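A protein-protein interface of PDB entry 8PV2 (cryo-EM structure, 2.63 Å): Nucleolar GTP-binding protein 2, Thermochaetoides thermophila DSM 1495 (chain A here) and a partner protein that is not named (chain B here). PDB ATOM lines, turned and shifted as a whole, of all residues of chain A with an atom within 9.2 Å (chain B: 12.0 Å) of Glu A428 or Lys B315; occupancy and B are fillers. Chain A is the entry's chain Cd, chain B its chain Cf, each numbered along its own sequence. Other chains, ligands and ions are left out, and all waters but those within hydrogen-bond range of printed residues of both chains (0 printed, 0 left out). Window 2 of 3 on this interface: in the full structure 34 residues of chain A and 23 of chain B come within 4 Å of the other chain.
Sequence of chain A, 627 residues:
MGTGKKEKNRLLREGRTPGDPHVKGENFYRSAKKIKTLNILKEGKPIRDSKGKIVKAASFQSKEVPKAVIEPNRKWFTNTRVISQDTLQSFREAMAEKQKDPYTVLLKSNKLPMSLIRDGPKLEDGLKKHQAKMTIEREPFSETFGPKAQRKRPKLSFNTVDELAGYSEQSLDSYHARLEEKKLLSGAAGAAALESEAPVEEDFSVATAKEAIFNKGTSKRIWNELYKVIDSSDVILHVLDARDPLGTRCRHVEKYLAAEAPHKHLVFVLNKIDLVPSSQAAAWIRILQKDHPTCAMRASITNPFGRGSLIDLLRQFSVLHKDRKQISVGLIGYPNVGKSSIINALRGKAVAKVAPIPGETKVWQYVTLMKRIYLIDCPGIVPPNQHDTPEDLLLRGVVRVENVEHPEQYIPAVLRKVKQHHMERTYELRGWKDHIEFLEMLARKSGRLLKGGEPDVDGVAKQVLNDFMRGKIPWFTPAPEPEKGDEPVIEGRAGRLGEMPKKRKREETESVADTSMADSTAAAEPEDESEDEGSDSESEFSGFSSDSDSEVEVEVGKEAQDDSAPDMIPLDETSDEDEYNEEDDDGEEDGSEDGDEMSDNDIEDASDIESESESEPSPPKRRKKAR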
ATOM      1  N   GLN A 420      18.859 -14.841 -17.755  1.00  0.00           N
ATOM      2  CA  GLN A 420      20.174 -15.464 -17.862  1.00  0.00           C
ATOM      3  C   GLN A 420      20.990 -15.279 -16.590  1.00  0.00           C
ATOM      4  O   GLN A 420      21.620 -16.226 -16.111  1.00  0.00           O
ATOM      5  CB  GLN A 420      20.929 -14.901 -19.064  1.00  0.00           C
ATOM      6  CG  GLN A 420      22.221 -15.638 -19.357  1.00  0.00           C
ATOM      7  CD  GLN A 420      22.906 -15.144 -20.606  1.00  0.00           C
ATOM      8  OE1 GLN A 420      22.730 -13.998 -21.013  1.00  0.00           O
ATOM      9  NE2 GLN A 420      23.682 -16.015 -21.237  1.00  0.00           N
ATOM     10  N   HIS A 421      20.975 -14.074 -16.019  1.00  0.00           N
ATOM     11  CA  HIS A 421      21.776 -13.820 -14.826  1.00  0.00           C
ATOM     12  C   HIS A 421      21.208 -14.547 -13.614  1.00  0.00           C
ATOM     13  O   HIS A 421      21.948 -14.874 -12.678  1.00  0.00           O
ATOM     14  CB  HIS A 421      21.887 -12.314 -14.577  1.00  0.00           C
ATOM     15  CG  HIS A 421      20.590 -11.648 -14.243  1.00  0.00           C
ATOM     16  ND1 HIS A 421      19.591 -11.455 -15.172  1.00  0.00           N
ATOM     17  CD2 HIS A 421      20.141 -11.099 -13.090  1.00  0.00           C
ATOM     18  CE1 HIS A 421      18.574 -10.837 -14.601  1.00  0.00           C
ATOM     19  NE2 HIS A 421      18.883 -10.607 -13.338  1.00  0.00           N
ATOM     20  N   HIS A 422      19.908 -14.849 -13.632  1.00  0.00           N
ATOM     21  CA  HIS A 422      19.329 -15.671 -12.575  1.00  0.00           C
ATOM     22  C   HIS A 422      19.870 -17.099 -12.629  1.00  0.00           C
ATOM     23  O   HIS A 422      20.231 -17.672 -11.597  1.00  0.00           O
ATOM     24  CB  HIS A 422      17.803 -15.656 -12.669  1.00  0.00           C
ATOM     25  CG  HIS A 422      17.180 -14.370 -12.220  1.00  0.00           C
ATOM     26  ND1 HIS A 422      16.022 -13.868 -12.775  1.00  0.00           N
ATOM     27  CD2 HIS A 422      17.561 -13.475 -11.278  1.00  0.00           C
ATOM     28  CE1 HIS A 422      15.713 -12.726 -12.189  1.00  0.00           C
ATOM     29  NE2 HIS A 422      16.631 -12.465 -11.277  1.00  0.00           N
ATOM     30  N   MET A 423      19.965 -17.679 -13.832  1.00  0.00           N
ATOM     31  CA  MET A 423      20.584 -18.997 -13.991  1.00  0.00           C
ATOM     32  C   MET A 423      22.057 -18.966 -13.604  1.00  0.00           C
ATOM     33  O   MET A 423      22.574 -19.909 -12.990  1.00  0.00           O
ATOM     34  CB  MET A 423      20.442 -19.483 -15.435  1.00  0.00           C
ATOM     35  CG  MET A 423      19.033 -19.762 -15.903  1.00  0.00           C
ATOM     36  SD  MET A 423      18.186 -21.053 -14.978  1.00  0.00           S
ATOM     37  CE  MET A 423      19.083 -22.501 -15.483  1.00  0.00           C
ATOM     38  N   GLU A 424      22.749 -17.891 -13.985  1.00  0.00           N
ATOM     39  CA  GLU A 424      24.174 -17.779 -13.700  1.00  0.00           C
ATOM     40  C   GLU A 424      24.443 -17.698 -12.205  1.00  0.00           C
ATOM     41  O   GLU A 424      25.376 -18.331 -11.705  1.00  0.00           O
ATOM     42  CB  GLU A 424      24.760 -16.571 -14.422  1.00  0.00           C
ATOM     43  CG  GLU A 424      24.796 -16.729 -15.927  1.00  0.00           C
ATOM     44  CD  GLU A 424      25.071 -15.426 -16.636  1.00  0.00           C
ATOM     45  OE1 GLU A 424      24.935 -14.365 -15.995  1.00  0.00           O
ATOM     46  OE2 GLU A 424      25.421 -15.462 -17.833  1.00  0.00           O
ATOM     47  N   ARG A 425      23.640 -16.934 -11.466  1.00  0.00           N
ATOM     48  CA  ARG A 425      23.845 -16.888 -10.023  1.00  0.00           C
ATOM     49  C   ARG A 425      23.280 -18.126  -9.335  1.00  0.00           C
ATOM     50  O   ARG A 425      23.693 -18.460  -8.219  1.00  0.00           O
ATOM     51  CB  ARG A 425      23.248 -15.614  -9.435  1.00  0.00           C
ATOM     52  CG  ARG A 425      23.971 -14.364  -9.899  1.00  0.00           C
ATOM     53  CD  ARG A 425      23.354 -13.113  -9.317  1.00  0.00           C
ATOM     54  NE  ARG A 425      22.014 -12.863  -9.824  1.00  0.00           N
ATOM     55  CZ  ARG A 425      21.214 -11.911  -9.366  1.00  0.00           C
ATOM     56  NH1 ARG A 425      21.599 -11.089  -8.406  1.00  0.00           N
ATOM     57  NH2 ARG A 425      19.993 -11.788  -9.877  1.00  0.00           N
ATOM     58  N   THR A 426      22.335 -18.820  -9.976  1.00  0.00           N
ATOM     59  CA  THR A 426      21.807 -20.045  -9.385  1.00  0.00           C
ATOM     60  C   THR A 426      22.836 -21.162  -9.418  1.00  0.00           C
ATOM     61  O   THR A 426      23.058 -21.841  -8.409  1.00  0.00           O
ATOM     62  CB  THR A 426      20.534 -20.476 -10.113  1.00  0.00           C
ATOM     63  OG1 THR A 426      19.548 -19.444 -10.000  1.00  0.00           O
ATOM     64  CG2 THR A 426      19.981 -21.753  -9.512  1.00  0.00           C
ATOM     65  N   TYR A 427      23.488 -21.362 -10.559  1.00  0.00           N
ATOM     66  CA  TYR A 427      24.413 -22.475 -10.708  1.00  0.00           C
ATOM     67  C   TYR A 427      25.878 -22.058 -10.666  1.00  0.00           C
ATOM     68  O   TYR A 427      26.746 -22.924 -10.819  1.00  0.00           O
ATOM     69  CB  TYR A 427      24.109 -23.234 -11.997  1.00  0.00           C
ATOM     70  CG  TYR A 427      22.813 -24.000 -11.920  1.00  0.00           C
ATOM     71  CD1 TYR A 427      22.694 -25.108 -11.097  1.00  0.00           C
ATOM     72  CD2 TYR A 427      21.703 -23.611 -12.658  1.00  0.00           C
ATOM     73  CE1 TYR A 427      21.514 -25.806 -11.010  1.00  0.00           C
ATOM     74  CE2 TYR A 427      20.518 -24.304 -12.577  1.00  0.00           C
ATOM     75  CZ  TYR A 427      20.431 -25.402 -11.753  1.00  0.00           C
ATOM     76  OH  TYR A 427      19.255 -26.104 -11.666  1.00  0.00           O
ATOM     77  N   GLU A 428      26.169 -20.772 -10.433  1.00  0.00           N
ATOM     78  CA  GLU A 428      27.529 -20.214 -10.422  1.00  0.00           C
ATOM     79  C   GLU A 428      28.295 -20.573 -11.693  1.00  0.00           C
ATOM     80  O   GLU A 428      29.463 -20.960 -11.665  1.00  0.00           O
ATOM     81  CB  GLU A 428      28.297 -20.646  -9.173  1.00  0.00           C
ATOM     82  CG  GLU A 428      28.027 -19.783  -7.957  1.00  0.00           C
ATOM     83  CD  GLU A 428      26.854 -20.267  -7.135  1.00  0.00           C
ATOM     84  OE1 GLU A 428      26.150 -21.195  -7.583  1.00  0.00           O
ATOM     85  OE2 GLU A 428      26.635 -19.714  -6.038  1.00  0.00           O
ATOM     86  N   LEU A 429      27.610 -20.435 -12.823  1.00  0.00           N
ATOM     87  CA  LEU A 429      28.105 -20.896 -14.108  1.00  0.00           C
ATOM     88  C   LEU A 429      27.792 -19.839 -15.152  1.00  0.00           C
ATOM     89  O   LEU A 429      26.719 -19.236 -15.140  1.00  0.00           O
ATOM     90  CB  LEU A 429      27.456 -22.234 -14.482  1.00  0.00           C
ATOM     91  CG  LEU A 429      28.149 -23.173 -15.458  1.00  0.00           C
ATOM     92  CD1 LEU A 429      29.253 -23.930 -14.760  1.00  0.00           C
ATOM     93  CD2 LEU A 429      27.137 -24.124 -16.053  1.00  0.00           C
ATOM     94  N   ARG A 430      28.730 -19.616 -16.069  1.00  0.00           N
ATOM     95  CA  ARG A 430      28.504 -18.613 -17.099  1.00  0.00           C
ATOM     96  C   ARG A 430      29.320 -18.957 -18.333  1.00  0.00           C
ATOM     97  O   ARG A 430      30.299 -19.703 -18.264  1.00  0.00           O
ATOM     98  CB  ARG A 430      28.856 -17.206 -16.605  1.00  0.00           C
ATOM     99  CG  ARG A 430      30.152 -17.122 -15.823  1.00  0.00           C
ATOM    100  CD  ARG A 430      30.265 -15.790 -15.099  1.00  0.00           C
ATOM    101  NE  ARG A 430      29.125 -15.551 -14.223  1.00  0.00           N
ATOM    102  CZ  ARG A 430      29.002 -16.055 -13.001  1.00  0.00           C
ATOM    103  NH1 ARG A 430      29.942 -16.820 -12.471  1.00  0.00           N
ATOM    104  NH2 ARG A 430      27.909 -15.782 -12.293  1.00  0.00           N
ATOM    105  N   GLY A 431      28.902 -18.397 -19.463  1.00  0.00           N
ATOM    106  CA  GLY A 431      29.652 -18.523 -20.694  1.00  0.00           C
ATOM    107  C   GLY A 431      29.140 -19.535 -21.690  1.00  0.00           C
ATOM    108  O   GLY A 431      29.844 -19.828 -22.662  1.00  0.00           O
ATOM    109  N   TRP A 432      27.944 -20.079 -21.496  1.00  0.00           N
ATOM    110  CA  TRP A 432      27.413 -21.037 -22.453  1.00  0.00           C
ATOM    111  C   TRP A 432      26.744 -20.314 -23.614  1.00  0.00           C
ATOM    112  O   TRP A 432      26.285 -19.177 -23.484  1.00  0.00           O
ATOM    113  CB  TRP A 432      26.421 -21.987 -21.779  1.00  0.00           C
ATOM    114  CG  TRP A 432      25.161 -21.343 -21.274  1.00  0.00           C
ATOM    115  CD1 TRP A 432      24.028 -21.078 -21.990  1.00  0.00           C
ATOM    116  CD2 TRP A 432      24.897 -20.910 -19.935  1.00  0.00           C
ATOM    117  NE1 TRP A 432      23.085 -20.495 -21.185  1.00  0.00           N
ATOM    118  CE2 TRP A 432      23.591 -20.382 -19.918  1.00  0.00           C
ATOM    119  CE3 TRP A 432      25.637 -20.913 -18.753  1.00  0.00           C
ATOM    120  CZ2 TRP A 432      23.014 -19.862 -18.768  1.00  0.00           C
ATOM    121  CZ3 TRP A 432      25.062 -20.399 -17.612  1.00  0.00           C
ATOM    122  CH2 TRP A 432      23.765 -19.879 -17.627  1.00  0.00           C
ATOM    123  N   PHE A 438      25.382 -25.648 -21.901  1.00  0.00           N
ATOM    124  CA  PHE A 438      25.030 -25.301 -20.526  1.00  0.00           C
ATOM    125  C   PHE A 438      24.934 -26.547 -19.648  1.00  0.00           C
ATOM    126  O   PHE A 438      25.504 -26.598 -18.548  1.00  0.00           O
ATOM    127  CB  PHE A 438      23.711 -24.524 -20.515  1.00  0.00           C
ATOM    128  CG  PHE A 438      23.042 -24.481 -19.175  1.00  0.00           C
ATOM    129  CD1 PHE A 438      23.533 -23.670 -18.171  1.00  0.00           C
ATOM    130  CD2 PHE A 438      21.925 -25.254 -18.917  1.00  0.00           C
ATOM    131  CE1 PHE A 438      22.924 -23.630 -16.939  1.00  0.00           C
ATOM    132  CE2 PHE A 438      21.317 -25.221 -17.684  1.00  0.00           C
ATOM    133  CZ  PHE A 438      21.818 -24.407 -16.696  1.00  0.00           C
ATOM    134  N   MET A 441      28.521 -28.136 -19.181  1.00  0.00           N
ATOM    135  CA  MET A 441      29.333 -27.412 -18.206  1.00  0.00           C
ATOM    136  C   MET A 441      28.829 -27.640 -16.790  1.00  0.00           C
ATOM    137  O   MET A 441      29.627 -27.810 -15.861  1.00  0.00           O
ATOM    138  CB  MET A 441      29.374 -25.919 -18.531  1.00  0.00           C
ATOM    139  CG  MET A 441      29.983 -25.575 -19.878  1.00  0.00           C
ATOM    140  SD  MET A 441      30.026 -23.806 -20.237  1.00  0.00           S
ATOM    141  CE  MET A 441      30.169 -23.108 -18.597  1.00  0.00           C
ATOM    142  N   LEU A 442      27.507 -27.659 -16.603  1.00  0.00           N
ATOM    143  CA  LEU A 442      26.963 -27.941 -15.276  1.00  0.00           C
ATOM    144  C   LEU A 442      27.289 -29.363 -14.828  1.00  0.00           C
ATOM    145  O   LEU A 442      27.589 -29.595 -13.651  1.00  0.00           O
ATOM    146  CB  LEU A 442      25.455 -27.700 -15.269  1.00  0.00           C
ATOM    147  CG  LEU A 442      24.749 -27.791 -13.915  1.00  0.00           C
ATOM    148  CD1 LEU A 442      25.506 -27.043 -12.831  1.00  0.00           C
ATOM    149  CD2 LEU A 442      23.332 -27.270 -14.033  1.00  0.00           C
ATOM    150  N   LYS A 445      30.889 -29.474 -13.820  1.00  0.00           N
ATOM    151  CA  LYS A 445      31.088 -28.767 -12.563  1.00  0.00           C
ATOM    152  C   LYS A 445      30.608 -29.595 -11.380  1.00  0.00           C
ATOM    153  O   LYS A 445      31.279 -29.654 -10.343  1.00  0.00           O
ATOM    154  CB  LYS A 445      30.366 -27.423 -12.597  1.00  0.00           C
ATOM    155  CG  LYS A 445      30.502 -26.654 -11.312  1.00  0.00           C
ATOM    156  CD  LYS A 445      29.511 -25.528 -11.215  1.00  0.00           C
ATOM    157  CE  LYS A 445      29.572 -24.916  -9.834  1.00  0.00           C
ATOM    158  NZ  LYS A 445      28.475 -23.952  -9.607  1.00  0.00           N
ATOM    159  N   ASP A 467      14.438 -28.224 -10.174  1.00  0.00           N
ATOM    160  CA  ASP A 467      14.724 -26.948  -9.523  1.00  0.00           C
ATOM    161  C   ASP A 467      13.812 -25.846 -10.045  1.00  0.00           C
ATOM    162  O   ASP A 467      13.368 -24.981  -9.282  1.00  0.00           O
ATOM    163  CB  ASP A 467      16.187 -26.568  -9.736  1.00  0.00           C
ATOM    164  CG  ASP A 467      17.140 -27.497  -9.023  1.00  0.00           C
ATOM    165  OD1 ASP A 467      16.678 -28.296  -8.184  1.00  0.00           O
ATOM    166  OD2 ASP A 467      18.354 -27.423  -9.294  1.00  0.00           O
ATOM    167  N   GLY A 471      10.469 -24.241  -7.073  1.00  0.00           N
ATOM    168  CA  GLY A 471      10.835 -22.965  -6.486  1.00  0.00           C
ATOM    169  C   GLY A 471      12.280 -22.835  -6.060  1.00  0.00           C
ATOM    170  O   GLY A 471      12.555 -22.328  -4.966  1.00  0.00           O
ATOM    171  N   LYS A 472      13.215 -23.291  -6.894  1.00  0.00           N
ATOM    172  CA  LYS A 472      14.635 -23.125  -6.626  1.00  0.00           C
ATOM    173  C   LYS A 472      15.333 -22.209  -7.616  1.00  0.00           C
ATOM    174  O   LYS A 472      16.434 -21.738  -7.325  1.00  0.00           O
ATOM    175  CB  LYS A 472      15.340 -24.487  -6.619  1.00  0.00           C
ATOM    176  CG  LYS A 472      14.905 -25.378  -5.479  1.00  0.00           C
ATOM    177  CD  LYS A 472      15.656 -26.687  -5.476  1.00  0.00           C
ATOM    178  CE  LYS A 472      15.129 -27.606  -4.398  1.00  0.00           C
ATOM    179  NZ  LYS A 472      15.415 -27.064  -3.045  1.00  0.00           N
ATOM    180  N   ILE A 473      14.726 -21.952  -8.770  1.00  0.00           N
ATOM    181  CA  ILE A 473      15.220 -20.982  -9.736  1.00  0.00           C
ATOM    182  C   ILE A 473      14.178 -19.878  -9.840  1.00  0.00           C
ATOM    183  O   ILE A 473      13.001 -20.174 -10.048  1.00  0.00           O
ATOM    184  CB  ILE A 473      15.476 -21.605 -11.119  1.00  0.00           C
ATOM    185  CG1 ILE A 473      16.225 -22.925 -10.986  1.00  0.00           C
ATOM    186  CG2 ILE A 473      16.277 -20.662 -11.962  1.00  0.00           C
ATOM    187  CD1 ILE A 473      16.286 -23.713 -12.268  1.00  0.00           C
ATOM    188  N   PRO A 474      14.554 -18.609  -9.691  1.00  0.00           N
ATOM    189  CA  PRO A 474      13.558 -17.530  -9.737  1.00  0.00           C
ATOM    190  C   PRO A 474      13.051 -17.278 -11.150  1.00  0.00           C
ATOM    191  O   PRO A 474      13.832 -17.079 -12.081  1.00  0.00           O
ATOM    192  CB  PRO A 474      14.322 -16.319  -9.191  1.00  0.00           C
ATOM    193  CG  PRO A 474      15.748 -16.636  -9.428  1.00  0.00           C
ATOM    194  CD  PRO A 474      15.883 -18.116  -9.298  1.00  0.00           C
ATOM    195  N   THR B 311       9.508 -12.236   0.690  1.00  0.00           N
ATOM    196  CA  THR B 311       9.618 -13.208  -0.383  1.00  0.00           C
ATOM    197  C   THR B 311      10.737 -14.201  -0.091  1.00  0.00           C
ATOM    198  O   THR B 311      11.585 -13.985   0.778  1.00  0.00           O
ATOM    199  CB  THR B 311       9.859 -12.517  -1.723  1.00  0.00           C
ATOM    200  OG1 THR B 311      10.903 -11.548  -1.592  1.00  0.00           O
ATOM    201  CG2 THR B 311       8.603 -11.820  -2.179  1.00  0.00           C
ATOM    202  N   ARG B 312      10.718 -15.315  -0.818  1.00  0.00           N
ATOM    203  CA  ARG B 312      11.711 -16.357  -0.609  1.00  0.00           C
ATOM    204  C   ARG B 312      13.078 -15.892  -1.091  1.00  0.00           C
ATOM    205  O   ARG B 312      13.237 -15.469  -2.239  1.00  0.00           O
ATOM    206  CB  ARG B 312      11.291 -17.636  -1.332  1.00  0.00           C
ATOM    207  CG  ARG B 312      12.213 -18.805  -1.080  1.00  0.00           C
ATOM    208  CD  ARG B 312      11.585 -20.109  -1.492  1.00  0.00           C
ATOM    209  NE  ARG B 312      12.438 -21.240  -1.153  1.00  0.00           N
ATOM    210  CZ  ARG B 312      12.463 -21.834   0.031  1.00  0.00           C
ATOM    211  NH1 ARG B 312      11.678 -21.442   1.019  1.00  0.00           N
ATOM    212  NH2 ARG B 312      13.293 -22.853   0.227  1.00  0.00           N
ATOM    213  N   LYS B 313      14.069 -15.969  -0.203  1.00  0.00           N
ATOM    214  CA  LYS B 313      15.413 -15.471  -0.491  1.00  0.00           C
ATOM    215  C   LYS B 313      16.163 -16.522  -1.305  1.00  0.00           C
ATOM    216  O   LYS B 313      16.976 -17.295  -0.798  1.00  0.00           O
ATOM    217  CB  LYS B 313      16.153 -15.133   0.795  1.00  0.00           C
ATOM    218  CG  LYS B 313      15.378 -14.279   1.780  1.00  0.00           C
ATOM    219  CD  LYS B 313      14.873 -12.998   1.154  1.00  0.00           C
ATOM    220  CE  LYS B 313      13.995 -12.234   2.125  1.00  0.00           C
ATOM    221  NZ  LYS B 313      13.214 -11.176   1.447  1.00  0.00           N
ATOM    222  N   MET B 314      15.862 -16.544  -2.599  1.00  0.00           N
ATOM    223  CA  MET B 314      16.402 -17.578  -3.468  1.00  0.00           C
ATOM    224  C   MET B 314      17.880 -17.342  -3.746  1.00  0.00           C
ATOM    225  O   MET B 314      18.395 -16.232  -3.608  1.00  0.00           O
ATOM    226  CB  MET B 314      15.619 -17.642  -4.778  1.00  0.00           C
ATOM    227  CG  MET B 314      14.332 -18.442  -4.670  1.00  0.00           C
ATOM    228  SD  MET B 314      13.199 -18.193  -6.046  1.00  0.00           S
ATOM    229  CE  MET B 314      12.226 -16.822  -5.436  1.00  0.00           C
ATOM    230  N   LYS B 315      18.564 -18.421  -4.130  1.00  0.00           N
ATOM    231  CA  LYS B 315      19.987 -18.341  -4.440  1.00  0.00           C
ATOM    232  C   LYS B 315      20.234 -17.509  -5.691  1.00  0.00           C
ATOM    233  O   LYS B 315      21.255 -16.824  -5.800  1.00  0.00           O
ATOM    234  CB  LYS B 315      20.551 -19.751  -4.608  1.00  0.00           C
ATOM    235  CG  LYS B 315      22.053 -19.835  -4.766  1.00  0.00           C
ATOM    236  CD  LYS B 315      22.477 -21.269  -5.029  1.00  0.00           C
ATOM    237  CE  LYS B 315      23.982 -21.422  -4.991  1.00  0.00           C
ATOM    238  NZ  LYS B 315      24.404 -22.801  -5.360  1.00  0.00           N
ATOM    239  N   GLY B 316      19.302 -17.551  -6.644  1.00  0.00           N
ATOM    240  CA  GLY B 316      19.461 -16.802  -7.875  1.00  0.00           C
ATOM    241  C   GLY B 316      19.228 -15.315  -7.732  1.00  0.00           C
ATOM    242  O   GLY B 316      19.614 -14.551  -8.621  1.00  0.00           O
ATOM    243  N   LEU B 317      18.606 -14.886  -6.638  1.00  0.00           N
ATOM    244  CA  LEU B 317      18.332 -13.477  -6.400  1.00  0.00           C
ATOM    245  C   LEU B 317      19.359 -12.810  -5.501  1.00  0.00           C
ATOM    246  O   LEU B 317      19.128 -11.686  -5.052  1.00  0.00           O
ATOM    247  CB  LEU B 317      16.938 -13.309  -5.797  1.00  0.00           C
ATOM    248  CG  LEU B 317      15.768 -13.685  -6.700  1.00  0.00           C
ATOM    249  CD1 LEU B 317      14.470 -13.446  -5.979  1.00  0.00           C
ATOM    250  CD2 LEU B 317      15.821 -12.870  -7.967  1.00  0.00           C
ATOM    251  N   LYS B 318      20.480 -13.465  -5.225  1.00  0.00           N
ATOM    252  CA  LYS B 318      21.517 -12.912  -4.365  1.00  0.00           C
ATOM    253  C   LYS B 318      22.730 -12.557  -5.211  1.00  0.00           C
ATOM    254  O   LYS B 318      23.126 -13.330  -6.088  1.00  0.00           O
ATOM    255  CB  LYS B 318      21.903 -13.896  -3.262  1.00  0.00           C
ATOM    256  CG  LYS B 318      20.770 -14.249  -2.328  1.00  0.00           C
ATOM    257  CD  LYS B 318      21.226 -15.241  -1.279  1.00  0.00           C
ATOM    258  CE  LYS B 318      20.120 -15.519  -0.278  1.00  0.00           C
ATOM    259  NZ  LYS B 318      20.537 -16.502   0.756  1.00  0.00           N
ATOM    260  N   ARG B 319      23.311 -11.392  -4.943  1.00  0.00           N
ATOM    261  CA  ARG B 319      24.435 -10.885  -5.723  1.00  0.00           C
ATOM    262  C   ARG B 319      25.691 -11.710  -5.469  1.00  0.00           C
ATOM    263  O   ARG B 319      26.301 -11.612  -4.405  1.00  0.00           O
ATOM    264  CB  ARG B 319      24.710  -9.414  -5.395  1.00  0.00           C
ATOM    265  CG  ARG B 319      23.776  -8.407  -6.061  1.00  0.00           C
ATOM    266  CD  ARG B 319      22.462  -8.261  -5.303  1.00  0.00           C
ATOM    267  NE  ARG B 319      22.674  -7.690  -3.978  1.00  0.00           N
ATOM    268  CZ  ARG B 319      21.767  -7.678  -3.010  1.00  0.00           C
ATOM    269  NH1 ARG B 319      20.570  -8.214  -3.177  1.00  0.00           N
ATOM    270  NH2 ARG B 319      22.074  -7.120  -1.842  1.00  0.00           N
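Among the printed residues, pairs that only touch across the chains: His A422 with Gly B316 (3.5 Å), His A422 with Leu B317 (3.4 Å), Arg A425 with Lys B315 (3.8 Å), Arg A425 with Lys B318 (3.2 Å), Arg A425 with Arg B319 (3.9 Å), Thr A426 with Gly B316 (3.4 Å), Gly A471 with Arg B312 (3.97 Å), Pro A474 with Met B314 (3.8 Å) and Pro A474 with Leu B317 (3.9 Å).
The backbone carbonyl oxygen (O) of His A422 lies within hydrogen-bond range of the side-chain hydroxyl (OG1) of Thr A426, at 2.5 Å.
O of His A421 lies close to NE of Arg A425 (3.5 Å).
Of the printed residues of chain B, Arg A425 touches Lys B315 (3.8 Å), Gly B316 (3.1 Å), Lys B318 (3.2 Å) and Arg B319 (3.9 Å).
Thr A426 touches just these residues of chain B: Lys B315 and Gly B316.
Printed residues of chain B within 4 Å of Glu A428: Lys B315 (3.3 Å).
No residue of chain B comes within 4 Å of Arg A430.
Of the printed residues of chain A, Arg B312 touches Gly A471 (3.97 Å).
Printed residues of chain A within 4 Å of Lys B315: Arg A425, Thr A426 and Glu A428.
Gly B316 touches just these residues of chain A: His A422 (3.5 Å), Arg A425 (3.1 Å) and Thr A426 (3.4 Å).
Of the printed residues of chain A, Leu B317 touches His A422 and Pro A474.
Of the printed residues of chain A, Lys B318 touches Arg A425 (3.2 Å).
Of the printed residues of chain A, Arg B319 touches Arg A425.
The nearest residue of chain B that does not touch Glu A428 is Lys B318 (7.3 Å).
The nearest residue of chain A that does not touch Lys B315 is Lys A472 (5.1 Å).
NH2 of Arg A425 sits at hydrogen-bond distance from O of Gly B316 (3.1 Å).
The backbone carbonyl oxygen (O) of Thr A426 lies within hydrogen-bond range of the side-chain amino group (NZ) of Lys B315, 3.5 Å away.
The side-chain amino group of Lys B315 is in salt-bridge range of the side-chain carboxylate of Glu A428 (3.3 Å).
Printed residues of chain B that touch a printed residue of chain A: Arg B312, Met B314, Lys B315, Gly B316, Leu B317, Lys B318 and Arg B319.
Hydrophobic or aromatic side chains of chain B that line the printed part of chain A: Met B314 and Leu B317.
Hydrophobic or aromatic side chains of chain A that line the printed part of chain B: His A422 and Pro A474.
Along chain A the printed residues that touch a printed residue of chain B span positions 422 to 474.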
